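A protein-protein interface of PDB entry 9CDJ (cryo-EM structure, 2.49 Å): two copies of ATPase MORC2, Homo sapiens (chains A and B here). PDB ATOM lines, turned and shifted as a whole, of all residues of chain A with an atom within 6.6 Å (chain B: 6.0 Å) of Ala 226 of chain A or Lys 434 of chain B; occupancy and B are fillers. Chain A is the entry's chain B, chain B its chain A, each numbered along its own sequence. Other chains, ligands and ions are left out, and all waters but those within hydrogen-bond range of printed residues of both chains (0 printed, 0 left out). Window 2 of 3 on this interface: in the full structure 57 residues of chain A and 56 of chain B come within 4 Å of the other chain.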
ATOM      1  N   GLU A  27     -27.896 -32.748  14.225  1.00  0.00           N
ATOM      2  CA  GLU A  27     -28.014 -31.343  14.580  1.00  0.00           C
ATOM      3  C   GLU A  27     -26.715 -30.591  14.330  1.00  0.00           C
ATOM      4  O   GLU A  27     -26.667 -29.371  14.515  1.00  0.00           O
ATOM      5  CB  GLU A  27     -28.444 -31.202  16.044  1.00  0.00           C
ATOM      6  CG  GLU A  27     -27.324 -31.389  17.063  1.00  0.00           C
ATOM      7  CD  GLU A  27     -26.705 -30.081  17.525  1.00  0.00           C
ATOM      8  OE1 GLU A  27     -25.754 -30.129  18.332  1.00  0.00           O
ATOM      9  OE2 GLU A  27     -27.164 -29.006  17.086  1.00  0.00           O
ATOM     10  N   MET A 207     -31.739 -22.825   4.469  1.00  0.00           N
ATOM     11  CA  MET A 207     -32.216 -22.171   5.675  1.00  0.00           C
ATOM     12  C   MET A 207     -33.558 -21.493   5.402  1.00  0.00           C
ATOM     13  O   MET A 207     -34.089 -21.520   4.288  1.00  0.00           O
ATOM     14  CB  MET A 207     -31.199 -21.147   6.173  1.00  0.00           C
ATOM     15  CG  MET A 207     -29.932 -21.764   6.750  1.00  0.00           C
ATOM     16  SD  MET A 207     -28.505 -20.662   6.918  1.00  0.00           S
ATOM     17  CE  MET A 207     -28.755 -19.451   5.621  1.00  0.00           C
ATOM     18  N   ASP A 208     -34.112 -20.875   6.447  1.00  0.00           N
ATOM     19  CA  ASP A 208     -35.392 -20.190   6.300  1.00  0.00           C
ATOM     20  C   ASP A 208     -35.340 -19.118   5.220  1.00  0.00           C
ATOM     21  O   ASP A 208     -36.347 -18.861   4.550  1.00  0.00           O
ATOM     22  CB  ASP A 208     -35.818 -19.593   7.646  1.00  0.00           C
ATOM     23  CG  ASP A 208     -34.992 -18.376   8.049  1.00  0.00           C
ATOM     24  OD1 ASP A 208     -35.204 -17.872   9.173  1.00  0.00           O
ATOM     25  OD2 ASP A 208     -34.120 -17.935   7.272  1.00  0.00           O
ATOM     26  N   ASN A 209     -34.183 -18.487   5.032  1.00  0.00           N
ATOM     27  CA  ASN A 209     -34.029 -17.422   4.048  1.00  0.00           C
ATOM     28  C   ASN A 209     -33.790 -17.945   2.637  1.00  0.00           C
ATOM     29  O   ASN A 209     -33.507 -17.145   1.738  1.00  0.00           O
ATOM     30  CB  ASN A 209     -32.879 -16.496   4.459  1.00  0.00           C
ATOM     31  CG  ASN A 209     -31.536 -17.197   4.463  1.00  0.00           C
ATOM     32  OD1 ASN A 209     -31.439 -18.381   4.146  1.00  0.00           O
ATOM     33  ND2 ASN A 209     -30.490 -16.465   4.825  1.00  0.00           N
ATOM     34  N   GLU A 211     -31.315 -19.725   1.528  1.00  0.00           N
ATOM     35  CA  GLU A 211     -29.912 -19.952   1.231  1.00  0.00           C
ATOM     36  C   GLU A 211     -29.450 -21.272   1.829  1.00  0.00           C
ATOM     37  O   GLU A 211     -30.021 -21.757   2.810  1.00  0.00           O
ATOM     38  CB  GLU A 211     -29.069 -18.804   1.782  1.00  0.00           C
ATOM     39  CG  GLU A 211     -29.349 -17.451   1.139  1.00  0.00           C
ATOM     40  CD  GLU A 211     -28.999 -17.403  -0.338  1.00  0.00           C
ATOM     41  OE1 GLU A 211     -29.112 -16.313  -0.937  1.00  0.00           O
ATOM     42  OE2 GLU A 211     -28.594 -18.443  -0.898  1.00  0.00           O
ATOM     43  N   PRO A 212     -28.414 -21.884   1.264  1.00  0.00           N
ATOM     44  CA  PRO A 212     -27.927 -23.156   1.800  1.00  0.00           C
ATOM     45  C   PRO A 212     -27.372 -22.999   3.207  1.00  0.00           C
ATOM     46  O   PRO A 212     -26.868 -21.946   3.598  1.00  0.00           O
ATOM     47  CB  PRO A 212     -26.825 -23.562   0.815  1.00  0.00           C
ATOM     48  CG  PRO A 212     -26.378 -22.287   0.204  1.00  0.00           C
ATOM     49  CD  PRO A 212     -27.599 -21.422   0.126  1.00  0.00           C
ATOM     50  N   GLU A 213     -27.481 -24.084   3.975  1.00  0.00           N
ATOM     51  CA  GLU A 213     -26.961 -24.070   5.337  1.00  0.00           C
ATOM     52  C   GLU A 213     -25.447 -23.924   5.361  1.00  0.00           C
ATOM     53  O   GLU A 213     -24.895 -23.375   6.321  1.00  0.00           O
ATOM     54  CB  GLU A 213     -27.374 -25.343   6.075  1.00  0.00           C
ATOM     55  CG  GLU A 213     -28.852 -25.670   5.996  1.00  0.00           C
ATOM     56  CD  GLU A 213     -29.264 -26.731   7.000  1.00  0.00           C
ATOM     57  OE1 GLU A 213     -28.693 -26.754   8.110  1.00  0.00           O
ATOM     58  OE2 GLU A 213     -30.160 -27.539   6.684  1.00  0.00           O
ATOM     59  N   LEU A 214     -24.762 -24.397   4.325  1.00  0.00           N
ATOM     60  CA  LEU A 214     -23.308 -24.347   4.255  1.00  0.00           C
ATOM     61  C   LEU A 214     -22.883 -23.124   3.452  1.00  0.00           C
ATOM     62  O   LEU A 214     -23.253 -22.983   2.282  1.00  0.00           O
ATOM     63  CB  LEU A 214     -22.752 -25.623   3.623  1.00  0.00           C
ATOM     64  CG  LEU A 214     -23.167 -26.922   4.310  1.00  0.00           C
ATOM     65  CD1 LEU A 214     -22.694 -28.124   3.515  1.00  0.00           C
ATOM     66  CD2 LEU A 214     -22.618 -26.967   5.723  1.00  0.00           C
ATOM     67  N   ASP A 215     -22.109 -22.248   4.085  1.00  0.00           N
ATOM     68  CA  ASP A 215     -21.591 -21.052   3.437  1.00  0.00           C
ATOM     69  C   ASP A 215     -20.236 -21.372   2.817  1.00  0.00           C
ATOM     70  O   ASP A 215     -19.286 -21.711   3.530  1.00  0.00           O
ATOM     71  CB  ASP A 215     -21.467 -19.909   4.444  1.00  0.00           C
ATOM     72  CG  ASP A 215     -20.912 -18.640   3.828  1.00  0.00           C
ATOM     73  OD1 ASP A 215     -20.645 -18.629   2.608  1.00  0.00           O
ATOM     74  OD2 ASP A 215     -20.741 -17.650   4.568  1.00  0.00           O
ATOM     75  N   GLN A 224     -18.210 -22.942   5.604  1.00  0.00           N
ATOM     76  CA  GLN A 224     -18.708 -22.402   6.857  1.00  0.00           C
ATOM     77  C   GLN A 224     -20.209 -22.633   6.979  1.00  0.00           C
ATOM     78  O   GLN A 224     -20.889 -23.012   6.024  1.00  0.00           O
ATOM     79  CB  GLN A 224     -18.393 -20.907   6.956  1.00  0.00           C
ATOM     80  CG  GLN A 224     -16.928 -20.600   7.184  1.00  0.00           C
ATOM     81  CD  GLN A 224     -16.638 -19.116   7.158  1.00  0.00           C
ATOM     82  OE1 GLN A 224     -16.381 -18.504   8.194  1.00  0.00           O
ATOM     83  NE2 GLN A 224     -16.677 -18.527   5.969  1.00  0.00           N
ATOM     84  N   MET A 225     -20.719 -22.399   8.183  1.00  0.00           N
ATOM     85  CA  MET A 225     -22.150 -22.412   8.442  1.00  0.00           C
ATOM     86  C   MET A 225     -22.702 -21.025   8.140  1.00  0.00           C
ATOM     87  O   MET A 225     -22.163 -20.022   8.618  1.00  0.00           O
ATOM     88  CB  MET A 225     -22.449 -22.787   9.894  1.00  0.00           C
ATOM     89  CG  MET A 225     -21.890 -24.131  10.325  1.00  0.00           C
ATOM     90  SD  MET A 225     -22.898 -25.532   9.820  1.00  0.00           S
ATOM     91  CE  MET A 225     -22.605 -26.651  11.185  1.00  0.00           C
ATOM     92  N   ALA A 226     -23.775 -20.972   7.356  1.00  0.00           N
ATOM     93  CA  ALA A 226     -24.347 -19.696   6.945  1.00  0.00           C
ATOM     94  C   ALA A 226     -25.053 -19.021   8.113  1.00  0.00           C
ATOM     95  O   ALA A 226     -26.287 -18.942   8.155  1.00  0.00           O
ATOM     96  CB  ALA A 226     -25.300 -19.903   5.769  1.00  0.00           C
ATOM     97  N   GLU A 227     -24.267 -18.508   9.056  1.00  0.00           N
ATOM     98  CA  GLU A 227     -24.820 -17.991  10.301  1.00  0.00           C
ATOM     99  C   GLU A 227     -23.774 -17.116  10.978  1.00  0.00           C
ATOM    100  O   GLU A 227     -22.587 -17.461  10.988  1.00  0.00           O
ATOM    101  CB  GLU A 227     -25.286 -19.182  11.154  1.00  0.00           C
ATOM    102  CG  GLU A 227     -24.200 -20.112  11.691  1.00  0.00           C
ATOM    103  CD  GLU A 227     -23.322 -19.542  12.804  1.00  0.00           C
ATOM    104  OE1 GLU A 227     -23.561 -18.391  13.223  1.00  0.00           O
ATOM    105  OE2 GLU A 227     -22.361 -20.225  13.207  1.00  0.00           O
ATOM    106  N   THR A 228     -24.211 -15.973  11.516  1.00  0.00           N
ATOM    107  CA  THR A 228     -23.297 -15.035  12.160  1.00  0.00           C
ATOM    108  C   THR A 228     -22.627 -15.665  13.376  1.00  0.00           C
ATOM    109  O   THR A 228     -23.275 -16.301  14.210  1.00  0.00           O
ATOM    110  CB  THR A 228     -24.048 -13.775  12.597  1.00  0.00           C
ATOM    111  OG1 THR A 228     -25.010 -14.125  13.603  1.00  0.00           O
ATOM    112  CG2 THR A 228     -24.762 -13.143  11.411  1.00  0.00           C
ATOM    113  N   ARG A 238     -18.160 -23.516  13.547  1.00  0.00           N
ATOM    114  CA  ARG A 238     -18.583 -22.609  12.487  1.00  0.00           C
ATOM    115  C   ARG A 238     -17.781 -22.755  11.204  1.00  0.00           C
ATOM    116  O   ARG A 238     -18.241 -22.289  10.156  1.00  0.00           O
ATOM    117  CB  ARG A 238     -18.488 -21.146  12.948  1.00  0.00           C
ATOM    118  CG  ARG A 238     -17.207 -20.810  13.680  1.00  0.00           C
ATOM    119  CD  ARG A 238     -17.047 -19.316  13.859  1.00  0.00           C
ATOM    120  NE  ARG A 238     -16.981 -18.612  12.584  1.00  0.00           N
ATOM    121  CZ  ARG A 238     -15.964 -18.686  11.736  1.00  0.00           C
ATOM    122  NH1 ARG A 238     -14.895 -19.420  12.000  1.00  0.00           N
ATOM    123  NH2 ARG A 238     -16.020 -18.006  10.596  1.00  0.00           N
ATOM    124  N   ALA B 431     -33.386 -30.433  15.375  1.00  0.00           N
ATOM    125  CA  ALA B 431     -32.631 -30.676  14.152  1.00  0.00           C
ATOM    126  C   ALA B 431     -31.997 -29.393  13.631  1.00  0.00           C
ATOM    127  O   ALA B 431     -30.827 -29.386  13.230  1.00  0.00           O
ATOM    128  CB  ALA B 431     -33.543 -31.297  13.094  1.00  0.00           C
ATOM    129  N   ASP B 432     -32.752 -28.298  13.627  1.00  0.00           N
ATOM    130  CA  ASP B 432     -32.247 -27.010  13.151  1.00  0.00           C
ATOM    131  C   ASP B 432     -31.526 -26.328  14.306  1.00  0.00           C
ATOM    132  O   ASP B 432     -32.126 -25.623  15.117  1.00  0.00           O
ATOM    133  CB  ASP B 432     -33.387 -26.152  12.614  1.00  0.00           C
ATOM    134  CG  ASP B 432     -32.947 -25.240  11.485  1.00  0.00           C
ATOM    135  OD1 ASP B 432     -31.725 -25.060  11.302  1.00  0.00           O
ATOM    136  OD2 ASP B 432     -33.826 -24.702  10.780  1.00  0.00           O
ATOM    137  N   ALA B 433     -30.211 -26.546  14.381  1.00  0.00           N
ATOM    138  CA  ALA B 433     -29.425 -25.951  15.457  1.00  0.00           C
ATOM    139  C   ALA B 433     -29.412 -24.431  15.372  1.00  0.00           C
ATOM    140  O   ALA B 433     -29.501 -23.755  16.401  1.00  0.00           O
ATOM    141  CB  ALA B 433     -27.999 -26.493  15.423  1.00  0.00           C
ATOM    142  N   LYS B 434     -29.299 -23.878  14.163  1.00  0.00           N
ATOM    143  CA  LYS B 434     -29.263 -22.427  14.010  1.00  0.00           C
ATOM    144  C   LYS B 434     -30.534 -21.789  14.555  1.00  0.00           C
ATOM    145  O   LYS B 434     -30.482 -20.844  15.352  1.00  0.00           O
ATOM    146  CB  LYS B 434     -29.072 -22.070  12.537  1.00  0.00           C
ATOM    147  CG  LYS B 434     -29.475 -20.650  12.180  1.00  0.00           C
ATOM    148  CD  LYS B 434     -29.007 -20.282  10.787  1.00  0.00           C
ATOM    149  CE  LYS B 434     -29.634 -18.983  10.315  1.00  0.00           C
ATOM    150  NZ  LYS B 434     -31.067 -19.157   9.949  1.00  0.00           N
ATOM    151  N   GLU B 435     -31.692 -22.301  14.144  1.00  0.00           N
ATOM    152  CA  GLU B 435     -32.947 -21.709  14.581  1.00  0.00           C
ATOM    153  C   GLU B 435     -33.252 -22.044  16.033  1.00  0.00           C
ATOM    154  O   GLU B 435     -33.905 -21.254  16.723  1.00  0.00           O
ATOM    155  CB  GLU B 435     -34.082 -22.171  13.670  1.00  0.00           C
ATOM    156  CG  GLU B 435     -34.084 -21.472  12.319  1.00  0.00           C
ATOM    157  CD  GLU B 435     -34.334 -19.980  12.429  1.00  0.00           C
ATOM    158  OE1 GLU B 435     -35.437 -19.586  12.861  1.00  0.00           O
ATOM    159  OE2 GLU B 435     -33.424 -19.197  12.082  1.00  0.00           O
ATOM    160  N   TYR B 436     -32.772 -23.186  16.527  1.00  0.00           N
ATOM    161  CA  TYR B 436     -32.910 -23.475  17.948  1.00  0.00           C
ATOM    162  C   TYR B 436     -32.122 -22.466  18.774  1.00  0.00           C
ATOM    163  O   TYR B 436     -32.595 -21.997  19.814  1.00  0.00           O
ATOM    164  CB  TYR B 436     -32.435 -24.896  18.247  1.00  0.00           C
ATOM    165  CG  TYR B 436     -32.288 -25.196  19.723  1.00  0.00           C
ATOM    166  CD1 TYR B 436     -33.211 -24.718  20.644  1.00  0.00           C
ATOM    167  CD2 TYR B 436     -31.214 -25.934  20.197  1.00  0.00           C
ATOM    168  CE1 TYR B 436     -33.082 -24.985  21.988  1.00  0.00           C
ATOM    169  CE2 TYR B 436     -31.074 -26.201  21.543  1.00  0.00           C
ATOM    170  CZ  TYR B 436     -32.010 -25.723  22.435  1.00  0.00           C
ATOM    171  OH  TYR B 436     -31.876 -25.986  23.778  1.00  0.00           O
ATOM    172  N   ARG B 437     -30.915 -22.116  18.323  1.00  0.00           N
ATOM    173  CA  ARG B 437     -30.135 -21.098  19.017  1.00  0.00           C
ATOM    174  C   ARG B 437     -30.780 -19.724  18.894  1.00  0.00           C
ATOM    175  O   ARG B 437     -30.710 -18.922  19.829  1.00  0.00           O
ATOM    176  CB  ARG B 437     -28.710 -21.059  18.473  1.00  0.00           C
ATOM    177  CG  ARG B 437     -27.838 -22.211  18.935  1.00  0.00           C
ATOM    178  CD  ARG B 437     -26.380 -21.964  18.596  1.00  0.00           C
ATOM    179  NE  ARG B 437     -26.167 -21.830  17.160  1.00  0.00           N
ATOM    180  CZ  ARG B 437     -25.895 -22.836  16.339  1.00  0.00           C
ATOM    181  NH1 ARG B 437     -25.796 -24.081  16.776  1.00  0.00           N
ATOM    182  NH2 ARG B 437     -25.718 -22.586  15.045  1.00  0.00           N
ATOM    183  N   HIS B 438     -31.396 -19.430  17.748  1.00  0.00           N
ATOM    184  CA  HIS B 438     -32.160 -18.193  17.623  1.00  0.00           C
ATOM    185  C   HIS B 438     -33.281 -18.145  18.656  1.00  0.00           C
ATOM    186  O   HIS B 438     -33.492 -17.123  19.321  1.00  0.00           O
ATOM    187  CB  HIS B 438     -32.727 -18.076  16.208  1.00  0.00           C
ATOM    188  CG  HIS B 438     -33.386 -16.762  15.926  1.00  0.00           C
ATOM    189  ND1 HIS B 438     -34.525 -16.652  15.158  1.00  0.00           N
ATOM    190  CD2 HIS B 438     -33.068 -15.504  16.310  1.00  0.00           C
ATOM    191  CE1 HIS B 438     -34.880 -15.383  15.080  1.00  0.00           C
ATOM    192  NE2 HIS B 438     -34.013 -14.665  15.770  1.00  0.00           N
ATOM    193  N   LEU B 439     -34.005 -19.255  18.806  1.00  0.00           N
ATOM    194  CA  LEU B 439     -35.058 -19.326  19.812  1.00  0.00           C
ATOM    195  C   LEU B 439     -34.490 -19.173  21.215  1.00  0.00           C
ATOM    196  O   LEU B 439     -35.100 -18.525  22.070  1.00  0.00           O
ATOM    197  CB  LEU B 439     -35.816 -20.646  19.685  1.00  0.00           C
ATOM    198  CG  LEU B 439     -37.021 -20.787  20.616  1.00  0.00           C
ATOM    199  CD1 LEU B 439     -38.213 -21.338  19.863  1.00  0.00           C
ATOM    200  CD2 LEU B 439     -36.686 -21.675  21.803  1.00  0.00           C
ATOM    201  N   ARG B 441     -31.792 -17.509  22.096  1.00  0.00           N
ATOM    202  CA  ARG B 441     -31.453 -16.102  22.289  1.00  0.00           C
ATOM    203  C   ARG B 441     -32.704 -15.266  22.532  1.00  0.00           C
ATOM    204  O   ARG B 441     -32.706 -14.373  23.391  1.00  0.00           O
ATOM    205  CB  ARG B 441     -30.686 -15.576  21.077  1.00  0.00           C
ATOM    206  CG  ARG B 441     -29.242 -16.037  21.010  1.00  0.00           C
ATOM    207  CD  ARG B 441     -28.455 -15.237  19.986  1.00  0.00           C
ATOM    208  NE  ARG B 441     -29.187 -15.079  18.735  1.00  0.00           N
ATOM    209  CZ  ARG B 441     -29.101 -15.902  17.699  1.00  0.00           C
ATOM    210  NH1 ARG B 441     -28.319 -16.970  17.723  1.00  0.00           N
ATOM    211  NH2 ARG B 441     -29.820 -15.649  16.609  1.00  0.00           N
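The backbone NH (N) of Ala 226 of chain A is in hydrogen-bond range of the backbone carbonyl oxygen (O) of Glu 213 of chain A, 2.8 Å away. NZ of Lys 434 of chain B is in salt-bridge range of OE2 of Glu 435 of chain B (3.2 Å).
Among the printed residues, pairs that only touch across the chains: Glu 27 of chain A with Ala 433 of chain B (3.1 Å), Asp 208 of chain A with Glu 435 of chain B (3.7 Å), Glu 27 of chain A with Ala 431 of chain B (3.7 Å), Glu 227 of chain A with Lys 434 of chain B (3.9 Å), Met 207 of chain A with Lys 434 of chain B (3.9 Å) and Ala 226 of chain A with Lys 434 of chain B (3.98 Å).
Of the printed residues of chain B, Ala 226 of chain A touches Lys 434 (3.98 Å). Of the printed residues of chain A, Lys 434 of chain B touches Met 207, Ala 226 and Glu 227. Printed residues of chain B within 4 Å of Glu 27 of chain A: Ala 431 (3.7 Å) and Ala 433 (3.1 Å). Of the printed residues of chain B, Glu 227 of chain A touches Lys 434. Glu 213 of chain A touches none of the printed residues of chain B. Asp 215 of chain A touches none of the printed residues of chain B.
Printed residues of chain A that touch a printed residue of chain B: Glu 27, Met 207, Asp 208, Ala 226 and Glu 227. Among the printed residues, 6 pairs touch across the chains. Among the printed residues, no Asp or Glu carboxylate lies within 4 Å of a Lys or Arg side-chain nitrogen of the other chain.
No position is printed for both chains. Of the 6 pairs that touch across the chains among the printed residues, none has its exchanged pair printed and touching as well.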
